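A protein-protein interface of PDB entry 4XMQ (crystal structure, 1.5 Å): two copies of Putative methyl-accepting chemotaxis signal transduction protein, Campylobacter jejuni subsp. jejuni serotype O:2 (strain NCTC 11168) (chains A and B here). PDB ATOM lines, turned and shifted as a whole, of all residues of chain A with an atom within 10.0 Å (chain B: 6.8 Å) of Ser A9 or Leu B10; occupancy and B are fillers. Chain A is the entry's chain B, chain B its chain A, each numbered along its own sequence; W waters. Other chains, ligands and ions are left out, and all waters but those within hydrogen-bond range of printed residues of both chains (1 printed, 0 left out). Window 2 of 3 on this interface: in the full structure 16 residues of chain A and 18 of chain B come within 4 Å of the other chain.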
ATOM      1  N   PRO A   4      29.572  27.391   4.330  1.00  0.00           N
ATOM      2  CA  PRO A   4      29.592  26.679   5.592  1.00  0.00           C
ATOM      3  C   PRO A   4      28.196  26.184   6.060  1.00  0.00           C
ATOM      4  O   PRO A   4      28.100  25.215   6.773  1.00  0.00           O
ATOM      5  CB  PRO A   4      30.148  27.726   6.569  1.00  0.00           C
ATOM      6  CG  PRO A   4      30.969  28.635   5.706  1.00  0.00           C
ATOM      7  CD  PRO A   4      30.227  28.718   4.416  1.00  0.00           C
ATOM      8  N   PHE A   5      27.148  26.928   5.689  1.00  0.00           N
ATOM      9  CA  PHE A   5      25.808  26.503   6.054  1.00  0.00           C
ATOM     10  C   PHE A   5      25.449  25.126   5.489  1.00  0.00           C
ATOM     11  O   PHE A   5      24.688  24.400   6.103  1.00  0.00           O
ATOM     12  CB  PHE A   5      24.758  27.539   5.665  1.00  0.00           C
ATOM     13  CG  PHE A   5      23.410  27.279   6.255  1.00  0.00           C
ATOM     14  CD1 PHE A   5      23.193  27.398   7.619  1.00  0.00           C
ATOM     15  CD2 PHE A   5      22.348  26.869   5.458  1.00  0.00           C
ATOM     16  CE1 PHE A   5      21.958  27.090   8.171  1.00  0.00           C
ATOM     17  CE2 PHE A   5      21.118  26.618   6.002  1.00  0.00           C
ATOM     18  CZ  PHE A   5      20.924  26.701   7.350  1.00  0.00           C
ATOM     19  N   THR A   6      26.060  24.769   4.358  1.00  0.00           N
ATOM     20  CA  THR A   6      25.794  23.472   3.729  1.00  0.00           C
ATOM     21  C   THR A   6      26.287  22.283   4.530  1.00  0.00           C
ATOM     22  O   THR A   6      25.936  21.134   4.222  1.00  0.00           O
ATOM     23  CB  THR A   6      26.300  23.401   2.268  1.00  0.00           C
ATOM     24  OG1 THR A   6      27.745  23.393   2.234  1.00  0.00           O
ATOM     25  CG2 THR A   6      25.739  24.542   1.453  1.00  0.00           C
ATOM     26  N   LYS A   7      27.118  22.533   5.549  1.00  0.00           N
ATOM     27  CA  LYS A   7      27.612  21.479   6.425  1.00  0.00           C
ATOM     28  C   LYS A   7      26.765  21.298   7.686  1.00  0.00           C
ATOM     29  O   LYS A   7      27.064  20.441   8.482  1.00  0.00           O
ATOM     30  CB  LYS A   7      29.080  21.779   6.797  1.00  0.00           C
ATOM     31  CG  LYS A   7      30.000  21.873   5.610  1.00  0.00           C
ATOM     32  CD  LYS A   7      31.405  22.309   6.102  1.00  0.00           C
ATOM     33  CE  LYS A   7      32.462  22.298   4.999  1.00  0.00           C
ATOM     34  NZ  LYS A   7      32.816  20.896   4.633  1.00  0.00           N
ATOM     35  N   THR A   8      25.713  22.105   7.886  1.00  0.00           N
ATOM     36  CA  THR A   8      24.879  21.998   9.072  1.00  0.00           C
ATOM     37  C   THR A   8      23.842  20.864   8.957  1.00  0.00           C
ATOM     38  O   THR A   8      23.416  20.499   7.841  1.00  0.00           O
ATOM     39  CB  THR A   8      24.112  23.308   9.385  1.00  0.00           C
ATOM     40  OG1 THR A   8      23.196  23.608   8.326  1.00  0.00           O
ATOM     41  CG2 THR A   8      25.058  24.472   9.563  1.00  0.00           C
ATOM     42  N   SER A   9      23.410  20.349  10.091  1.00  0.00           N
ATOM     43  CA  SER A   9      22.352  19.374  10.147  1.00  0.00           C
ATOM     44  C   SER A   9      21.036  20.015   9.692  1.00  0.00           C
ATOM     45  O   SER A   9      20.197  19.347   9.073  1.00  0.00           O
ATOM     46  CB  SER A   9      22.252  18.744  11.571  1.00  0.00           C
ATOM     47  OG  SER A   9      21.699  19.667  12.530  1.00  0.00           O
ATOM     48  N   LEU A  10      20.885  21.307   9.950  1.00  0.00           N
ATOM     49  CA  LEU A  10      19.698  22.013   9.548  1.00  0.00           C
ATOM     50  C   LEU A  10      19.605  22.089   8.026  1.00  0.00           C
ATOM     51  O   LEU A  10      18.511  21.910   7.461  1.00  0.00           O
ATOM     52  CB  LEU A  10      19.673  23.425  10.131  1.00  0.00           C
ATOM     53  CG  LEU A  10      18.548  24.346   9.713  1.00  0.00           C
ATOM     54  CD1 LEU A  10      17.197  23.764  10.107  1.00  0.00           C
ATOM     55  CD2 LEU A  10      18.692  25.746  10.296  1.00  0.00           C
ATOM     56  N   TYR A  11      20.720  22.354   7.335  1.00  0.00           N
ATOM     57  CA  TYR A  11      20.676  22.318   5.842  1.00  0.00           C
ATOM     58  C   TYR A  11      20.334  20.961   5.310  1.00  0.00           C
ATOM     59  O   TYR A  11      19.477  20.817   4.422  1.00  0.00           O
ATOM     60  CB  TYR A  11      22.022  22.741   5.295  1.00  0.00           C
ATOM     61  CG  TYR A  11      22.111  22.826   3.797  1.00  0.00           C
ATOM     62  CD1 TYR A  11      21.603  23.923   3.124  1.00  0.00           C
ATOM     63  CD2 TYR A  11      22.622  21.769   3.058  1.00  0.00           C
ATOM     64  CE1 TYR A  11      21.698  24.056   1.730  1.00  0.00           C
ATOM     65  CE2 TYR A  11      22.775  21.879   1.646  1.00  0.00           C
ATOM     66  CZ  TYR A  11      22.282  23.021   1.000  1.00  0.00           C
ATOM     67  OH  TYR A  11      22.378  23.158  -0.351  1.00  0.00           O
ATOM     68  N   GLU A  12      20.914  19.925   5.914  1.00  0.00           N
ATOM     69  CA  GLU A  12      20.698  18.563   5.449  1.00  0.00           C
ATOM     70  C   GLU A  12      19.218  18.190   5.590  1.00  0.00           C
ATOM     71  O   GLU A  12      18.617  17.571   4.683  1.00  0.00           O
ATOM     72  CB  GLU A  12      21.584  17.592   6.248  1.00  0.00           C
ATOM     73  CG  GLU A  12      21.369  16.129   5.912  1.00  0.00           C
ATOM     74  CD  GLU A  12      22.159  15.230   6.860  1.00  0.00           C
ATOM     75  OE1 GLU A  12      22.188  15.526   8.059  1.00  0.00           O
ATOM     76  OE2 GLU A  12      22.709  14.234   6.396  1.00  0.00           O
ATOM     77  N   SER A  13      18.620  18.603   6.682  1.00  0.00           N
ATOM     78  CA  SER A  13      17.231  18.220   6.941  1.00  0.00           C
ATOM     79  C   SER A  13      16.276  19.075   6.096  1.00  0.00           C
ATOM     80  O   SER A  13      15.181  18.616   5.709  1.00  0.00           O
ATOM     81  CB  SER A  13      16.892  18.324   8.409  1.00  0.00           C
ATOM     82  OG  SER A  13      16.680  19.628   8.786  1.00  0.00           O
ATOM     83  N   THR A  14      16.683  20.310   5.833  1.00  0.00           N
ATOM     84  CA  THR A  14      15.961  21.165   4.916  1.00  0.00           C
ATOM     85  C   THR A  14      15.897  20.564   3.517  1.00  0.00           C
ATOM     86  O   THR A  14      14.811  20.466   2.951  1.00  0.00           O
ATOM     87  CB  THR A  14      16.568  22.554   4.898  1.00  0.00           C
ATOM     88  OG1 THR A  14      16.457  23.108   6.218  1.00  0.00           O
ATOM     89  CG2 THR A  14      15.896  23.479   3.843  1.00  0.00           C
ATOM     90  N   LEU A  15      17.030  20.126   2.984  1.00  0.00           N
ATOM     91  CA  LEU A  15      17.085  19.477   1.689  1.00  0.00           C
ATOM     92  C   LEU A  15      16.285  18.177   1.663  1.00  0.00           C
ATOM     93  O   LEU A  15      15.613  17.897   0.694  1.00  0.00           O
ATOM     94  CB  LEU A  15      18.504  19.229   1.206  1.00  0.00           C
ATOM     95  CG  LEU A  15      19.004  20.321   0.250  1.00  0.00           C
ATOM     96  CD1 LEU A  15      18.922  21.677   0.934  1.00  0.00           C
ATOM     97  CD2 LEU A  15      20.425  19.950  -0.171  1.00  0.00           C
ATOM     98  N   LYS A  16      16.347  17.410   2.763  1.00  0.00           N
ATOM     99  CA  LYS A  16      15.566  16.188   2.839  1.00  0.00           C
ATOM    100  C   LYS A  16      14.071  16.518   2.702  1.00  0.00           C
ATOM    101  O   LYS A  16      13.343  15.782   2.007  1.00  0.00           O
ATOM    102  CB  LYS A  16      15.853  15.408   4.124  1.00  0.00           C
ATOM    103  CG  LYS A  16      14.907  14.223   4.311  1.00  0.00           C
ATOM    104  CD  LYS A  16      15.489  13.143   5.194  1.00  0.00           C
ATOM    105  CE  LYS A  16      14.467  12.040   5.501  1.00  0.00           C
ATOM    106  NZ  LYS A  16      13.930  11.382   4.265  1.00  0.00           N
ATOM    107  N   ASN A  17      13.607  17.584   3.369  1.00  0.00           N
ATOM    108  CA  ASN A  17      12.171  17.959   3.319  1.00  0.00           C
ATOM    109  C   ASN A  17      11.820  18.395   1.886  1.00  0.00           C
ATOM    110  O   ASN A  17      10.753  18.048   1.364  1.00  0.00           O
ATOM    111  CB  ASN A  17      11.841  19.108   4.293  1.00  0.00           C
ATOM    112  CG  ASN A  17      10.434  19.793   4.047  1.00  0.00           C
ATOM    113  OD1 ASN A  17       9.380  19.237   4.368  1.00  0.00           O
ATOM    114  ND2 ASN A  17      10.451  21.063   3.539  1.00  0.00           N
ATOM    115  N   ILE A 247      15.915  28.882   2.705  1.00  0.00           N
ATOM    116  CA  ILE A 247      16.754  27.711   2.978  1.00  0.00           C
ATOM    117  C   ILE A 247      17.749  28.008   4.109  1.00  0.00           C
ATOM    118  O   ILE A 247      17.919  27.216   5.017  1.00  0.00           O
ATOM    119  CB  ILE A 247      17.527  27.283   1.708  1.00  0.00           C
ATOM    120  CG1 ILE A 247      16.505  26.845   0.586  1.00  0.00           C
ATOM    121  CG2 ILE A 247      18.555  26.219   2.035  1.00  0.00           C
ATOM    122  CD1 ILE A 247      15.707  25.619   0.959  1.00  0.00           C
ATOM    123  N   LYS A 249      17.904  31.138   6.548  1.00  0.00           N
ATOM    124  CA  LYS A 249      17.318  32.395   6.978  1.00  0.00           C
ATOM    125  C   LYS A 249      18.404  33.300   7.572  1.00  0.00           C
ATOM    126  O   LYS A 249      18.998  32.947   8.621  1.00  0.00           O
ATOM    127  CB  LYS A 249      16.200  32.163   8.015  1.00  0.00           C
ATOM    128  CG  LYS A 249      15.083  31.264   7.496  1.00  0.00           C
ATOM    129  CD  LYS A 249      14.021  31.085   8.585  1.00  0.00           C
ATOM    130  CE  LYS A 249      13.300  29.751   8.467  1.00  0.00           C
ATOM    131  NZ  LYS A 249      13.250  29.292   7.061  1.00  0.00           N
ATOM    132  N   PHE B   5      19.592  29.123  20.287  1.00  0.00           N
ATOM    133  CA  PHE B   5      19.196  29.601  18.979  1.00  0.00           C
ATOM    134  C   PHE B   5      19.241  28.473  17.995  1.00  0.00           C
ATOM    135  O   PHE B   5      18.332  28.339  17.169  1.00  0.00           O
ATOM    136  CB  PHE B   5      20.166  30.693  18.529  1.00  0.00           C
ATOM    137  CG  PHE B   5      19.901  31.248  17.153  1.00  0.00           C
ATOM    138  CD1 PHE B   5      19.049  32.336  16.970  1.00  0.00           C
ATOM    139  CD2 PHE B   5      20.474  30.654  16.047  1.00  0.00           C
ATOM    140  CE1 PHE B   5      18.834  32.864  15.717  1.00  0.00           C
ATOM    141  CE2 PHE B   5      20.263  31.196  14.787  1.00  0.00           C
ATOM    142  CZ  PHE B   5      19.433  32.281  14.627  1.00  0.00           C
ATOM    143  N   THR B   6      20.277  27.661  18.075  1.00  0.00           N
ATOM    144  CA  THR B   6      20.427  26.570  17.114  1.00  0.00           C
ATOM    145  C   THR B   6      19.377  25.498  17.340  1.00  0.00           C
ATOM    146  O   THR B   6      18.737  25.009  16.384  1.00  0.00           O
ATOM    147  CB  THR B   6      21.810  25.939  17.193  1.00  0.00           C
ATOM    148  OG1 THR B   6      22.760  26.937  16.831  1.00  0.00           O
ATOM    149  CG2 THR B   6      21.944  24.823  16.263  1.00  0.00           C
ATOM    150  N   LYS B   7      19.215  25.075  18.573  1.00  0.00           N
ATOM    151  CA  LYS B   7      18.211  24.048  18.866  1.00  0.00           C
ATOM    152  C   LYS B   7      16.836  24.501  18.446  1.00  0.00           C
ATOM    153  O   LYS B   7      16.070  23.718  17.856  1.00  0.00           O
ATOM    154  CB  LYS B   7      18.242  23.623  20.359  1.00  0.00           C
ATOM    155  CG  LYS B   7      17.353  22.418  20.641  1.00  0.00           C
ATOM    156  CD  LYS B   7      17.464  21.956  22.099  1.00  0.00           C
ATOM    157  CE  LYS B   7      16.665  20.679  22.332  1.00  0.00           C
ATOM    158  NZ  LYS B   7      16.721  20.257  23.757  1.00  0.00           N
ATOM    159  N   THR B   8      16.524  25.765  18.704  1.00  0.00           N
ATOM    160  CA  THR B   8      15.244  26.318  18.314  1.00  0.00           C
ATOM    161  C   THR B   8      15.054  26.265  16.811  1.00  0.00           C
ATOM    162  O   THR B   8      13.994  25.892  16.303  1.00  0.00           O
ATOM    163  CB  THR B   8      15.082  27.743  18.832  1.00  0.00           C
ATOM    164  OG1 THR B   8      15.049  27.697  20.270  1.00  0.00           O
ATOM    165  CG2 THR B   8      13.826  28.362  18.329  1.00  0.00           C
ATOM    166  N   SER B   9      16.108  26.579  16.072  1.00  0.00           N
ATOM    167  CA  SER B   9      16.039  26.574  14.615  1.00  0.00           C
ATOM    168  C   SER B   9      15.785  25.153  14.111  1.00  0.00           C
ATOM    169  O   SER B   9      15.014  24.947  13.162  1.00  0.00           O
ATOM    170  CB  SER B   9      17.322  27.158  14.009  1.00  0.00           C
ATOM    171  OG  SER B   9      18.387  26.268  14.081  1.00  0.00           O
ATOM    172  N   LEU B  10      16.414  24.170  14.735  1.00  0.00           N
ATOM    173  CA  LEU B  10      16.216  22.750  14.365  1.00  0.00           C
ATOM    174  C   LEU B  10      14.789  22.305  14.716  1.00  0.00           C
ATOM    175  O   LEU B  10      14.111  21.592  13.924  1.00  0.00           O
ATOM    176  CB  LEU B  10      17.227  21.856  15.079  1.00  0.00           C
ATOM    177  CG  LEU B  10      18.691  22.012  14.678  1.00  0.00           C
ATOM    178  CD1 LEU B  10      19.594  21.185  15.560  1.00  0.00           C
ATOM    179  CD2 LEU B  10      18.938  21.578  13.245  1.00  0.00           C
ATOM    180  N   TYR B  11      14.294  22.746  15.855  1.00  0.00           N
ATOM    181  CA  TYR B  11      12.974  22.358  16.303  1.00  0.00           C
ATOM    182  C   TYR B  11      11.945  22.956  15.355  1.00  0.00           C
ATOM    183  O   TYR B  11      11.035  22.238  14.918  1.00  0.00           O
ATOM    184  CB  TYR B  11      12.733  22.821  17.753  1.00  0.00           C
ATOM    185  CG  TYR B  11      11.336  22.506  18.260  1.00  0.00           C
ATOM    186  CD1 TYR B  11      11.011  21.233  18.681  1.00  0.00           C
ATOM    187  CD2 TYR B  11      10.378  23.456  18.291  1.00  0.00           C
ATOM    188  CE1 TYR B  11       9.742  20.939  19.121  1.00  0.00           C
ATOM    189  CE2 TYR B  11       9.080  23.188  18.736  1.00  0.00           C
ATOM    190  CZ  TYR B  11       8.778  21.933  19.138  1.00  0.00           C
ATOM    191  OH  TYR B  11       7.497  21.667  19.587  1.00  0.00           O
ATOM    192  N   GLU B  12      12.027  24.268  15.079  1.00  0.00           N
ATOM    193  CA  GLU B  12      11.081  24.905  14.201  1.00  0.00           C
ATOM    194  C   GLU B  12      11.051  24.299  12.805  1.00  0.00           C
ATOM    195  O   GLU B  12       9.982  24.169  12.178  1.00  0.00           O
ATOM    196  CB  GLU B  12      11.244  26.419  14.149  1.00  0.00           C
ATOM    197  CG  GLU B  12      10.916  27.076  15.482  1.00  0.00           C
ATOM    198  CD  GLU B  12      10.863  28.601  15.410  1.00  0.00           C
ATOM    199  OE1 GLU B  12      11.037  29.176  14.303  1.00  0.00           O
ATOM    200  OE2 GLU B  12      10.649  29.227  16.479  1.00  0.00           O
ATOM    201  N   SER B  13      12.200  23.886  12.323  1.00  0.00           N
ATOM    202  CA  SER B  13      12.345  23.250  11.019  1.00  0.00           C
ATOM    203  C   SER B  13      11.673  21.899  10.972  1.00  0.00           C
ATOM    204  O   SER B  13      10.926  21.604  10.048  1.00  0.00           O
ATOM    205  CB  SER B  13      13.826  23.117  10.640  1.00  0.00           C
ATOM    206  OG  SER B  13      13.984  22.426   9.412  1.00  0.00           O
ATOM    207  N   THR B  14      11.976  21.058  11.954  1.00  0.00           N
ATOM    208  CA  THR B  14      11.438  19.681  11.946  1.00  0.00           C
ATOM    209  C   THR B  14       9.953  19.726  12.224  1.00  0.00           C
ATOM    210  O   THR B  14       9.182  18.944  11.643  1.00  0.00           O
ATOM    211  CB  THR B  14      12.162  18.729  12.904  1.00  0.00           C
ATOM    212  OG1 THR B  14      11.809  17.349  12.584  1.00  0.00           O
ATOM    213  CG2 THR B  14      11.833  19.027  14.307  1.00  0.00           C
ATOM    214  N   LEU B  15       9.505  20.712  13.011  1.00  0.00           N
ATOM    215  CA  LEU B  15       8.091  20.882  13.236  1.00  0.00           C
ATOM    216  C   LEU B  15       7.410  21.133  11.900  1.00  0.00           C
ATOM    217  O   LEU B  15       6.361  20.510  11.610  1.00  0.00           O
ATOM    218  CB  LEU B  15       7.790  21.992  14.211  1.00  0.00           C
ATOM    219  CG  LEU B  15       6.387  22.325  14.684  1.00  0.00           C
ATOM    220  CD1 LEU B  15       6.420  22.898  16.112  1.00  0.00           C
ATOM    221  CD2 LEU B  15       5.683  23.263  13.733  1.00  0.00           C
ATOM    222  N   ASP B 245      16.269  12.924  18.062  1.00  0.00           N
ATOM    223  CA  ASP B 245      17.729  13.084  17.782  1.00  0.00           C
ATOM    224  C   ASP B 245      18.021  14.262  16.858  1.00  0.00           C
ATOM    225  O   ASP B 245      19.049  14.916  16.984  1.00  0.00           O
ATOM    226  CB  ASP B 245      18.263  11.775  17.172  1.00  0.00           C
ATOM    227  CG  ASP B 245      18.435  10.647  18.216  1.00  0.00           C
ATOM    228  OD1 ASP B 245      18.304  10.854  19.447  1.00  0.00           O
ATOM    229  OD2 ASP B 245      18.678   9.506  17.800  1.00  0.00           O
ATOM    230  N   ILE B 246      17.077  14.588  15.968  1.00  0.00           N
ATOM    231  CA  ILE B 246      17.277  15.718  15.031  1.00  0.00           C
ATOM    232  C   ILE B 246      17.444  17.069  15.750  1.00  0.00           C
ATOM    233  O   ILE B 246      18.156  17.963  15.255  1.00  0.00           O
ATOM    234  CB  ILE B 246      16.127  15.785  13.940  1.00  0.00           C
ATOM    235  CG1 ILE B 246      16.453  16.813  12.838  1.00  0.00           C
ATOM    236  CG2 ILE B 246      14.766  16.047  14.582  1.00  0.00           C
ATOM    237  CD1 ILE B 246      15.597  16.675  11.602  1.00  0.00           C
ATOM    238  N   ILE B 247      16.801  17.233  16.905  1.00  0.00           N
ATOM    239  CA  ILE B 247      16.921  18.462  17.669  1.00  0.00           C
ATOM    240  C   ILE B 247      17.957  18.367  18.788  1.00  0.00           C
ATOM    241  O   ILE B 247      18.443  19.389  19.281  1.00  0.00           O
ATOM    242  CB  ILE B 247      15.590  18.973  18.205  1.00  0.00           C
ATOM    243  CG1 ILE B 247      15.066  18.090  19.341  1.00  0.00           C
ATOM    244  CG2 ILE B 247      14.589  19.064  17.055  1.00  0.00           C
ATOM    245  CD1 ILE B 247      13.802  18.608  20.041  1.00  0.00           C
ATOM    246  N   ASN B 248      18.299  17.143  19.176  1.00  0.00           N
ATOM    247  CA  ASN B 248      19.172  16.918  20.341  1.00  0.00           C
ATOM    248  C   ASN B 248      20.636  16.632  19.999  1.00  0.00           C
ATOM    249  O   ASN B 248      21.515  16.845  20.833  1.00  0.00           O
ATOM    250  CB  ASN B 248      18.611  15.738  21.150  1.00  0.00           C
ATOM    251  CG  ASN B 248      17.349  16.086  21.893  1.00  0.00           C
ATOM    252  OD1 ASN B 248      17.180  17.205  22.383  1.00  0.00           O
ATOM    253  ND2 ASN B 248      16.468  15.107  22.036  1.00  0.00           N
ATOM    254  N   LYS B 249      20.871  16.090  18.796  1.00  0.00           N
ATOM    255  CA  LYS B 249      22.183  15.701  18.303  1.00  0.00           C
ATOM    256  C   LYS B 249      22.498  16.486  17.021  1.00  0.00           C
ATOM    257  O   LYS B 249      22.342  17.727  16.983  1.00  0.00           O
ATOM    258  CB  LYS B 249      22.218  14.184  18.038  1.00  0.00           C
ATOM    259  CG  LYS B 249      21.876  13.304  19.251  1.00  0.00           C
ATOM    260  CD  LYS B 249      22.800  13.557  20.439  1.00  0.00           C
ATOM    261  CE  LYS B 249      22.492  12.662  21.634  1.00  0.00           C
ATOM    262  NZ  LYS B 249      23.364  13.015  22.790  1.00  0.00           N
HETATM  263  O   HOH W   1      13.269  22.836   6.697  1.00  0.00           O
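Of chain A, only Ser A9 (3.4 Å) and Leu A10 (3.7 Å) come within 4 Å of Leu B10.
Of chain A, only Leu A10 (3.8 Å) comes within 4 Å of Ser B9.
Printed residues of chain B within 4 Å of Leu A10: Ser B9 (3.8 Å), Leu B10 (3.7 Å) and Ser B13 (3.5 Å).
Printed residues of chain A within 4 Å of Ser B13: Leu A10 (3.5 Å) and Ser A13 (3.9 Å).
Lys A16 touches none of the printed residues of chain B.
Lys B7 touches none of the printed residues of chain A.
The nearest residue of chain B that does not touch Ser A9 is Ile B246 (4.8 Å).
The nearest printed residue of chain B that does not touch Ser A13 is Leu B10 (5.4 Å).
Water W1 bridges OG of Ser B13 and OG1 of Thr A14.
Hydrophobic or aromatic side chains of chain A within 4 Å of the printed part of chain B: Leu A10.
Printed residues of chain B that touch a printed residue of chain A: Ser B9, Leu B10, Ser B13 and Ile B246.
Along chain B the printed residues that touch a printed residue of chain A span positions 9 to 246.
Among the printed residues, no Asp or Glu carboxylate lies within 4 Å of a Lys or Arg side-chain nitrogen of the other chain.
Ser A9 touches Leu B10, and with the chains exchanged Leu A10 touches Ser B9.
Leu B10 touches its own counterpart, Leu A10.
Leu A10 touches Ser B13, but with the chains exchanged Ser A13 does not touch Leu B10 (5.4 Å).
Ser A13 touches its own counterpart, Ser B13.
The backbone carbonyl oxygen (O) of Thr B6 lies within hydrogen-bond range of the side-chain hydroxyl (OG) of Ser B9, 2.6 Å away.
The side-chain hydroxyl (OG) of Ser A13 is in hydrogen-bond range of the backbone carbonyl oxygen (O) of Leu A10 (3.2 Å).
OG1 of Thr A14 lies within hydrogen-bond range of O of Leu A10, 2.7 Å away.
Among the printed residues, pairs that only touch across the chains: Ser A9 with Leu B10 (3.4 Å), Leu A10 with Ser B13 (3.5 Å), Leu A10 with Leu B10 (3.7 Å), Ser A13 with Ile B246 (3.8 Å), Leu A10 with Ser B9 (3.8 Å) and Ser A13 with Ser B13 (3.9 Å).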
